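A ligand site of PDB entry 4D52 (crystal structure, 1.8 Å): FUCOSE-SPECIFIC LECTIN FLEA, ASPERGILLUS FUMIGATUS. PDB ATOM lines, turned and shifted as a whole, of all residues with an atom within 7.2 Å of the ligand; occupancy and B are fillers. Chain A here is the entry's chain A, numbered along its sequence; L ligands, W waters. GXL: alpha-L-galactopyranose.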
ATOM      1  N   HIS A  71      -8.129 -11.752   9.331  1.00  0.00           N
ATOM      2  CA  HIS A  71      -8.154 -10.296   9.457  1.00  0.00           C
ATOM      3  C   HIS A  71      -6.773  -9.813   9.891  1.00  0.00           C
ATOM      4  O   HIS A  71      -6.303 -10.196  10.961  1.00  0.00           O
ATOM      5  CB  HIS A  71      -9.185  -9.873  10.481  1.00  0.00           C
ATOM      6  CG  HIS A  71     -10.574 -10.368  10.203  1.00  0.00           C
ATOM      7  ND1 HIS A  71     -11.345  -9.885   9.166  1.00  0.00           N
ATOM      8  CD2 HIS A  71     -11.334 -11.287  10.845  1.00  0.00           C
ATOM      9  CE1 HIS A  71     -12.512 -10.508   9.163  1.00  0.00           C
ATOM     10  NE2 HIS A  71     -12.534 -11.350  10.185  1.00  0.00           N
ATOM     11  N   ILE A  72      -6.108  -9.029   9.064  1.00  0.00           N
ATOM     12  CA  ILE A  72      -4.809  -8.473   9.434  1.00  0.00           C
ATOM     13  C   ILE A  72      -4.897  -6.946   9.357  1.00  0.00           C
ATOM     14  O   ILE A  72      -5.541  -6.401   8.457  1.00  0.00           O
ATOM     15  CB  ILE A  72      -3.679  -8.982   8.513  1.00  0.00           C
ATOM     16  CG1 ILE A  72      -3.609 -10.511   8.507  1.00  0.00           C
ATOM     17  CG2 ILE A  72      -2.335  -8.406   8.942  1.00  0.00           C
ATOM     18  CD1 ILE A  72      -2.795 -11.079   7.357  1.00  0.00           C
ATOM     19  N   ARG A  73      -4.274  -6.261  10.313  1.00  0.00           N
ATOM     20  CA  ARG A  73      -4.221  -4.787  10.311  1.00  0.00           C
ATOM     21  C   ARG A  73      -2.781  -4.321  10.557  1.00  0.00           C
ATOM     22  O   ARG A  73      -2.144  -4.784  11.521  1.00  0.00           O
ATOM     23  CB  ARG A  73      -5.175  -4.265  11.384  1.00  0.00           C
ATOM     24  CG  ARG A  73      -6.624  -4.705  11.256  1.00  0.00           C
ATOM     25  CD  ARG A  73      -7.293  -4.028  10.059  1.00  0.00           C
ATOM     26  NE  ARG A  73      -8.707  -4.338   9.959  1.00  0.00           N
ATOM     27  CZ  ARG A  73      -9.238  -5.376   9.311  1.00  0.00           C
ATOM     28  NH1 ARG A  73      -8.466  -6.266   8.683  1.00  0.00           N
ATOM     29  NH2 ARG A  73     -10.553  -5.531   9.273  1.00  0.00           N
ATOM     30  N   TYR A  75      -0.159  -0.975  10.933  1.00  0.00           N
ATOM     31  CA  TYR A  75      -0.210   0.449  11.277  1.00  0.00           C
ATOM     32  C   TYR A  75       1.137   1.094  11.098  1.00  0.00           C
ATOM     33  O   TYR A  75       2.170   0.541  11.536  1.00  0.00           O
ATOM     34  CB  TYR A  75      -0.682   0.593  12.734  1.00  0.00           C
ATOM     35  CG  TYR A  75      -2.063   0.001  12.898  1.00  0.00           C
ATOM     36  CD1 TYR A  75      -3.214   0.735  12.543  1.00  0.00           C
ATOM     37  CD2 TYR A  75      -2.246  -1.309  13.383  1.00  0.00           C
ATOM     38  CE1 TYR A  75      -4.473   0.185  12.654  1.00  0.00           C
ATOM     39  CE2 TYR A  75      -3.505  -1.859  13.494  1.00  0.00           C
ATOM     40  CZ  TYR A  75      -4.615  -1.115  13.139  1.00  0.00           C
ATOM     41  OH  TYR A  75      -5.869  -1.688  13.256  1.00  0.00           O
ATOM     42  N   GLU A  85      -3.710   2.760   8.407  1.00  0.00           N
ATOM     43  CA  GLU A  85      -4.009   1.354   8.601  1.00  0.00           C
ATOM     44  C   GLU A  85      -4.141   0.685   7.239  1.00  0.00           C
ATOM     45  O   GLU A  85      -4.961   1.143   6.416  1.00  0.00           O
ATOM     46  CB  GLU A  85      -5.308   1.244   9.360  1.00  0.00           C
ATOM     47  CG  GLU A  85      -5.877  -0.156   9.540  1.00  0.00           C
ATOM     48  CD  GLU A  85      -7.243  -0.129  10.199  1.00  0.00           C
ATOM     49  OE1 GLU A  85      -8.138   0.613   9.713  1.00  0.00           O
ATOM     50  OE2 GLU A  85      -7.432  -0.821  11.218  1.00  0.00           O
ATOM     51  N   ALA A  87      -5.352  -2.747   5.740  1.00  0.00           N
ATOM     52  CA  ALA A  87      -6.227  -3.811   6.263  1.00  0.00           C
ATOM     53  C   ALA A  87      -6.385  -4.915   5.254  1.00  0.00           C
ATOM     54  O   ALA A  87      -6.480  -4.660   4.048  1.00  0.00           O
ATOM     55  CB  ALA A  87      -7.592  -3.247   6.628  1.00  0.00           C
ATOM     56  N   ASP A  89      -8.834  -8.403   4.815  1.00  0.00           N
ATOM     57  CA  ASP A  89      -9.813  -9.415   5.206  1.00  0.00           C
ATOM     58  C   ASP A  89      -9.904 -10.521   4.137  1.00  0.00           C
ATOM     59  O   ASP A  89      -9.866 -10.242   2.924  1.00  0.00           O
ATOM     60  CB  ASP A  89     -11.222  -8.838   5.411  1.00  0.00           C
ATOM     61  CG  ASP A  89     -11.268  -7.665   6.373  1.00  0.00           C
ATOM     62  OD1 ASP A  89     -10.751  -7.794   7.505  1.00  0.00           O
ATOM     63  OD2 ASP A  89     -11.869  -6.617   5.995  1.00  0.00           O
ATOM     64  N   TYR A  95      -6.758  -3.265   1.599  1.00  0.00           N
ATOM     65  CA  TYR A  95      -7.389  -1.981   1.381  1.00  0.00           C
ATOM     66  C   TYR A  95      -6.937  -0.986   2.453  1.00  0.00           C
ATOM     67  O   TYR A  95      -6.321  -1.365   3.468  1.00  0.00           O
ATOM     68  CB  TYR A  95      -8.926  -2.093   1.400  1.00  0.00           C
ATOM     69  CG  TYR A  95      -9.533  -2.616   2.696  1.00  0.00           C
ATOM     70  CD1 TYR A  95      -9.675  -3.982   2.917  1.00  0.00           C
ATOM     71  CD2 TYR A  95      -9.981  -1.742   3.682  1.00  0.00           C
ATOM     72  CE1 TYR A  95     -10.246  -4.457   4.092  1.00  0.00           C
ATOM     73  CE2 TYR A  95     -10.560  -2.215   4.850  1.00  0.00           C
ATOM     74  CZ  TYR A  95     -10.697  -3.572   5.052  1.00  0.00           C
ATOM     75  OH  TYR A  95     -11.268  -3.988   6.220  1.00  0.00           O
ATOM     76  N   ASN A  96      -7.245   0.285   2.220  1.00  0.00           N
ATOM     77  CA  ASN A  96      -6.880   1.320   3.170  1.00  0.00           C
ATOM     78  C   ASN A  96      -7.953   1.335   4.238  1.00  0.00           C
ATOM     79  O   ASN A  96      -9.137   1.506   3.955  1.00  0.00           O
ATOM     80  CB  ASN A  96      -6.728   2.685   2.488  1.00  0.00           C
ATOM     81  CG  ASN A  96      -5.434   2.815   1.707  1.00  0.00           C
ATOM     82  OD1 ASN A  96      -4.318   2.546   2.231  1.00  0.00           O
ATOM     83  ND2 ASN A  96      -5.545   3.262   0.459  1.00  0.00           N
ATOM     84  N   GLY A  97      -7.541   1.061   5.465  1.00  0.00           N
ATOM     85  CA  GLY A  97      -8.467   0.976   6.565  1.00  0.00           C
ATOM     86  C   GLY A  97      -8.986   2.311   7.055  1.00  0.00           C
ATOM     87  O   GLY A  97      -8.388   3.352   6.819  1.00  0.00           O
ATOM     88  N   GLY A  98     -10.106   2.252   7.745  1.00  0.00           N
ATOM     89  CA  GLY A  98     -10.809   3.442   8.205  1.00  0.00           C
ATOM     90  C   GLY A  98     -10.080   4.317   9.223  1.00  0.00           C
ATOM     91  O   GLY A  98     -10.449   5.445   9.396  1.00  0.00           O
ATOM     92  N   LEU A  99      -9.047   3.804   9.907  1.00  0.00           N
ATOM     93  CA  LEU A  99      -8.245   4.630  10.793  1.00  0.00           C
ATOM     94  C   LEU A  99      -7.735   5.897  10.104  1.00  0.00           C
ATOM     95  O   LEU A  99      -7.711   6.958  10.717  1.00  0.00           O
ATOM     96  CB  LEU A  99      -7.078   3.867  11.410  1.00  0.00           C
ATOM     97  CG  LEU A  99      -6.166   4.685  12.353  1.00  0.00           C
ATOM     98  CD1 LEU A  99      -6.931   5.288  13.529  1.00  0.00           C
ATOM     99  CD2 LEU A  99      -5.053   3.792  12.877  1.00  0.00           C
ATOM    100  N   GLY A 100      -7.329   5.797   8.847  1.00  0.00           N
ATOM    101  CA  GLY A 100      -6.818   6.945   8.095  1.00  0.00           C
ATOM    102  C   GLY A 100      -7.814   8.103   7.961  1.00  0.00           C
ATOM    103  O   GLY A 100      -7.403   9.276   7.908  1.00  0.00           O
ATOM    104  N   PHE A 116      -5.637  -6.726  18.400  1.00  0.00           N
ATOM    105  CA  PHE A 116      -7.048  -7.162  18.546  1.00  0.00           C
ATOM    106  C   PHE A 116      -7.267  -7.644  19.974  1.00  0.00           C
ATOM    107  O   PHE A 116      -6.462  -8.403  20.499  1.00  0.00           O
ATOM    108  CB  PHE A 116      -7.375  -8.327  17.609  1.00  0.00           C
ATOM    109  CG  PHE A 116      -7.684  -7.917  16.200  1.00  0.00           C
ATOM    110  CD1 PHE A 116      -8.882  -7.325  15.890  1.00  0.00           C
ATOM    111  CD2 PHE A 116      -6.768  -8.132  15.170  1.00  0.00           C
ATOM    112  CE1 PHE A 116      -9.181  -6.941  14.600  1.00  0.00           C
ATOM    113  CE2 PHE A 116      -7.050  -7.757  13.860  1.00  0.00           C
ATOM    114  CZ  PHE A 116      -8.264  -7.155  13.570  1.00  0.00           C
ATOM    115  N   ALA A 122     -16.999  -9.622  19.034  1.00  0.00           N
ATOM    116  CA  ALA A 122     -16.756  -8.952  17.757  1.00  0.00           C
ATOM    117  C   ALA A 122     -15.344  -8.379  17.735  1.00  0.00           C
ATOM    118  O   ALA A 122     -14.721  -8.243  18.775  1.00  0.00           O
ATOM    119  CB  ALA A 122     -17.782  -7.841  17.560  1.00  0.00           C
ATOM    120  N   LEU A 123     -14.860  -8.023  16.550  1.00  0.00           N
ATOM    121  CA  LEU A 123     -13.507  -7.491  16.378  1.00  0.00           C
ATOM    122  C   LEU A 123     -13.350  -6.112  17.056  1.00  0.00           C
ATOM    123  O   LEU A 123     -14.044  -5.162  16.722  1.00  0.00           O
ATOM    124  CB  LEU A 123     -13.130  -7.360  14.902  1.00  0.00           C
ATOM    125  CG  LEU A 123     -12.791  -8.578  14.031  1.00  0.00           C
ATOM    126  CD1 LEU A 123     -13.965  -9.516  13.794  1.00  0.00           C
ATOM    127  CD2 LEU A 123     -12.330  -8.080  12.682  1.00  0.00           C
ATOM    128  N   GLN A 124     -12.422  -6.028  18.005  1.00  0.00           N
ATOM    129  CA  GLN A 124     -12.103  -4.781  18.693  1.00  0.00           C
ATOM    130  C   GLN A 124     -10.616  -4.579  18.668  1.00  0.00           C
ATOM    131  O   GLN A 124      -9.865  -5.544  18.861  1.00  0.00           O
ATOM    132  CB  GLN A 124     -12.588  -4.855  20.131  1.00  0.00           C
ATOM    133  CG  GLN A 124     -14.116  -4.980  20.213  1.00  0.00           C
ATOM    134  CD  GLN A 124     -14.576  -5.092  21.649  1.00  0.00           C
ATOM    135  OE1 GLN A 124     -14.804  -6.183  22.142  1.00  0.00           O
ATOM    136  NE2 GLN A 124     -14.655  -3.972  22.324  1.00  0.00           N
ATOM    137  N   LEU A 125     -10.195  -3.341  18.388  1.00  0.00           N
ATOM    138  CA  LEU A 125      -8.788  -2.976  18.222  1.00  0.00           C
ATOM    139  C   LEU A 125      -8.433  -1.906  19.217  1.00  0.00           C
ATOM    140  O   LEU A 125      -9.224  -1.000  19.508  1.00  0.00           O
ATOM    141  CB  LEU A 125      -8.512  -2.463  16.809  1.00  0.00           C
ATOM    142  CG  LEU A 125      -8.502  -3.498  15.685  1.00  0.00           C
ATOM    143  CD1 LEU A 125      -8.853  -2.890  14.337  1.00  0.00           C
ATOM    144  CD2 LEU A 125      -7.143  -4.212  15.589  1.00  0.00           C
ATOM    145  N   TRP A 141     -11.090   0.942  18.252  1.00  0.00           N
ATOM    146  CA  TRP A 141     -12.141   0.612  17.312  1.00  0.00           C
ATOM    147  C   TRP A 141     -13.046  -0.399  17.981  1.00  0.00           C
ATOM    148  O   TRP A 141     -12.614  -1.504  18.341  1.00  0.00           O
ATOM    149  CB  TRP A 141     -11.572   0.050  16.030  1.00  0.00           C
ATOM    150  CG  TRP A 141     -12.634  -0.512  15.157  1.00  0.00           C
ATOM    151  CD1 TRP A 141     -13.129  -1.784  15.184  1.00  0.00           C
ATOM    152  CD2 TRP A 141     -13.347   0.181  14.131  1.00  0.00           C
ATOM    153  NE1 TRP A 141     -14.109  -1.926  14.237  1.00  0.00           N
ATOM    154  CE2 TRP A 141     -14.258  -0.735  13.577  1.00  0.00           C
ATOM    155  CE3 TRP A 141     -13.301   1.486  13.632  1.00  0.00           C
ATOM    156  CZ2 TRP A 141     -15.134  -0.392  12.545  1.00  0.00           C
ATOM    157  CZ3 TRP A 141     -14.148   1.832  12.583  1.00  0.00           C
ATOM    158  CH2 TRP A 141     -15.060   0.888  12.041  1.00  0.00           C
ATOM    159  N   GLY A 143     -16.277  -1.060  16.569  1.00  0.00           N
ATOM    160  CA  GLY A 143     -17.319  -1.334  15.582  1.00  0.00           C
ATOM    161  C   GLY A 143     -18.091  -0.133  15.058  1.00  0.00           C
ATOM    162  O   GLY A 143     -18.979  -0.304  14.231  1.00  0.00           O
ATOM    163  N   TRP A 146     -13.342   5.105  14.744  1.00  0.00           N
ATOM    164  CA  TRP A 146     -12.168   5.264  15.583  1.00  0.00           C
ATOM    165  C   TRP A 146     -12.319   6.414  16.566  1.00  0.00           C
ATOM    166  O   TRP A 146     -12.800   7.481  16.210  1.00  0.00           O
ATOM    167  CB  TRP A 146     -10.942   5.472  14.708  1.00  0.00           C
ATOM    168  CG  TRP A 146     -10.515   4.204  14.061  1.00  0.00           C
ATOM    169  CD1 TRP A 146     -10.898   3.726  12.810  1.00  0.00           C
ATOM    170  CD2 TRP A 146      -9.668   3.205  14.624  1.00  0.00           C
ATOM    171  NE1 TRP A 146     -10.303   2.509  12.585  1.00  0.00           N
ATOM    172  CE2 TRP A 146      -9.552   2.164  13.680  1.00  0.00           C
ATOM    173  CE3 TRP A 146      -8.997   3.093  15.858  1.00  0.00           C
ATOM    174  CZ2 TRP A 146      -8.756   1.041  13.904  1.00  0.00           C
ATOM    175  CZ3 TRP A 146      -8.211   1.980  16.080  1.00  0.00           C
ATOM    176  CH2 TRP A 146      -8.111   0.951  15.096  1.00  0.00           C
HETATM  177  C1  GXL L   1     -12.399  -2.255   8.824  1.00  0.00           C
HETATM  178  C2  GXL L   1     -11.446  -1.058   8.953  1.00  0.00           C
HETATM  179  C3  GXL L   1     -11.477  -0.472  10.363  1.00  0.00           C
HETATM  180  C4  GXL L   1     -11.181  -1.579  11.383  1.00  0.00           C
HETATM  181  C5  GXL L   1     -12.188  -2.732  11.200  1.00  0.00           C
HETATM  182  C6  GXL L   1     -11.955  -3.877  12.194  1.00  0.00           C
HETATM  183  O1  GXL L   1     -13.734  -1.766   8.964  1.00  0.00           O
HETATM  184  O2  GXL L   1     -11.753  -0.055   7.961  1.00  0.00           O
HETATM  185  O3  GXL L   1     -10.515   0.604  10.466  1.00  0.00           O
HETATM  186  O4  GXL L   1      -9.850  -2.047  11.191  1.00  0.00           O
HETATM  187  O5  GXL L   1     -12.108  -3.222   9.855  1.00  0.00           O
HETATM  188  O6  GXL L   1     -12.991  -4.886  12.124  1.00  0.00           O
HETATM  189  O   HOH W   1     -13.644  -6.040   9.212  1.00  0.00           O
HETATM  190  O   HOH W   2     -15.175  -3.900   8.079  1.00  0.00           O
HETATM  191  O   HOH W   3     -15.150  -4.402  13.474  1.00  0.00           O
HETATM  192  O   HOH W   4     -13.987   1.380   8.233  1.00  0.00           O
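The side-chain carboxylate of Glu 85 lies within hydrogen-bond range of an oxygen (O3) of the ligand (2.5 Å). The guanidinium group (NE) of Arg 73 lies within hydrogen-bond range of an oxygen (O4) of the ligand. O3 of the ligand sits at hydrogen-bond distance from NE1 of Trp 146. The backbone NH (N) of Gly 98 lies within hydrogen-bond range of an oxygen (O2) of the ligand, 2.8 Å away.
Tyr 95 touches the ligand (OH to C1, 3.3 Å). Gly 97 touches the ligand. N of Leu 99 touches O3 of the ligand, at 3.6 Å. Leu 123 touches the ligand. Leu 125 touches the ligand. Trp 141 touches the ligand. Hydrophobic or aromatic side chains within 4 Å of the ligand: Tyr 95, Leu 123, Leu 125, Trp 141 and Trp 146. Within 4 Å of the ligand: Arg 73, Glu 85, Tyr 95, Gly 97, Gly 98, Leu 99, Leu 123, Leu 125, Trp 141 and Trp 146. The nearest printed residue that does not touch the ligand is Tyr 75 (4.5 Å).
Water W3 lies within hydrogen-bond range of an oxygen (O6) of the ligand (2.6 Å) and the indole nitrogen (NE1) of Trp 141 (2.8 Å). Water W1 bridges NH2 of Arg 73 (3.1 Å) and O6 of the ligand (3.2 Å).
The side-chain carboxylate (OE2) of Glu 85 sits at hydrogen-bond distance from the side-chain hydroxyl (OH) of Tyr 75, at 2.7 Å. OD1 of Asp 89 lies within salt-bridge range of NH2 of Arg 73. NH2 of Arg 73 lies within hydrogen-bond range of OH of Tyr 95, 3.5 Å away. O of Leu 125 lies within hydrogen-bond range of N of Trp 141 (3.0 Å). The side-chain carboxylate of Glu 85 is in hydrogen-bond range of the backbone NH of Gly 98, at 3.2 Å. The backbone NH (N) of Gly 97 sits at hydrogen-bond distance from the backbone carbonyl oxygen (O) of Glu 85. The backbone carbonyl oxygen of Tyr 95 is in hydrogen-bond range of the backbone NH of Ala 87, at 2.8 Å. The backbone NH (N) of Leu 99 sits at hydrogen-bond distance from the side-chain carboxylate (OE1) of Glu 85 (3.3 Å).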
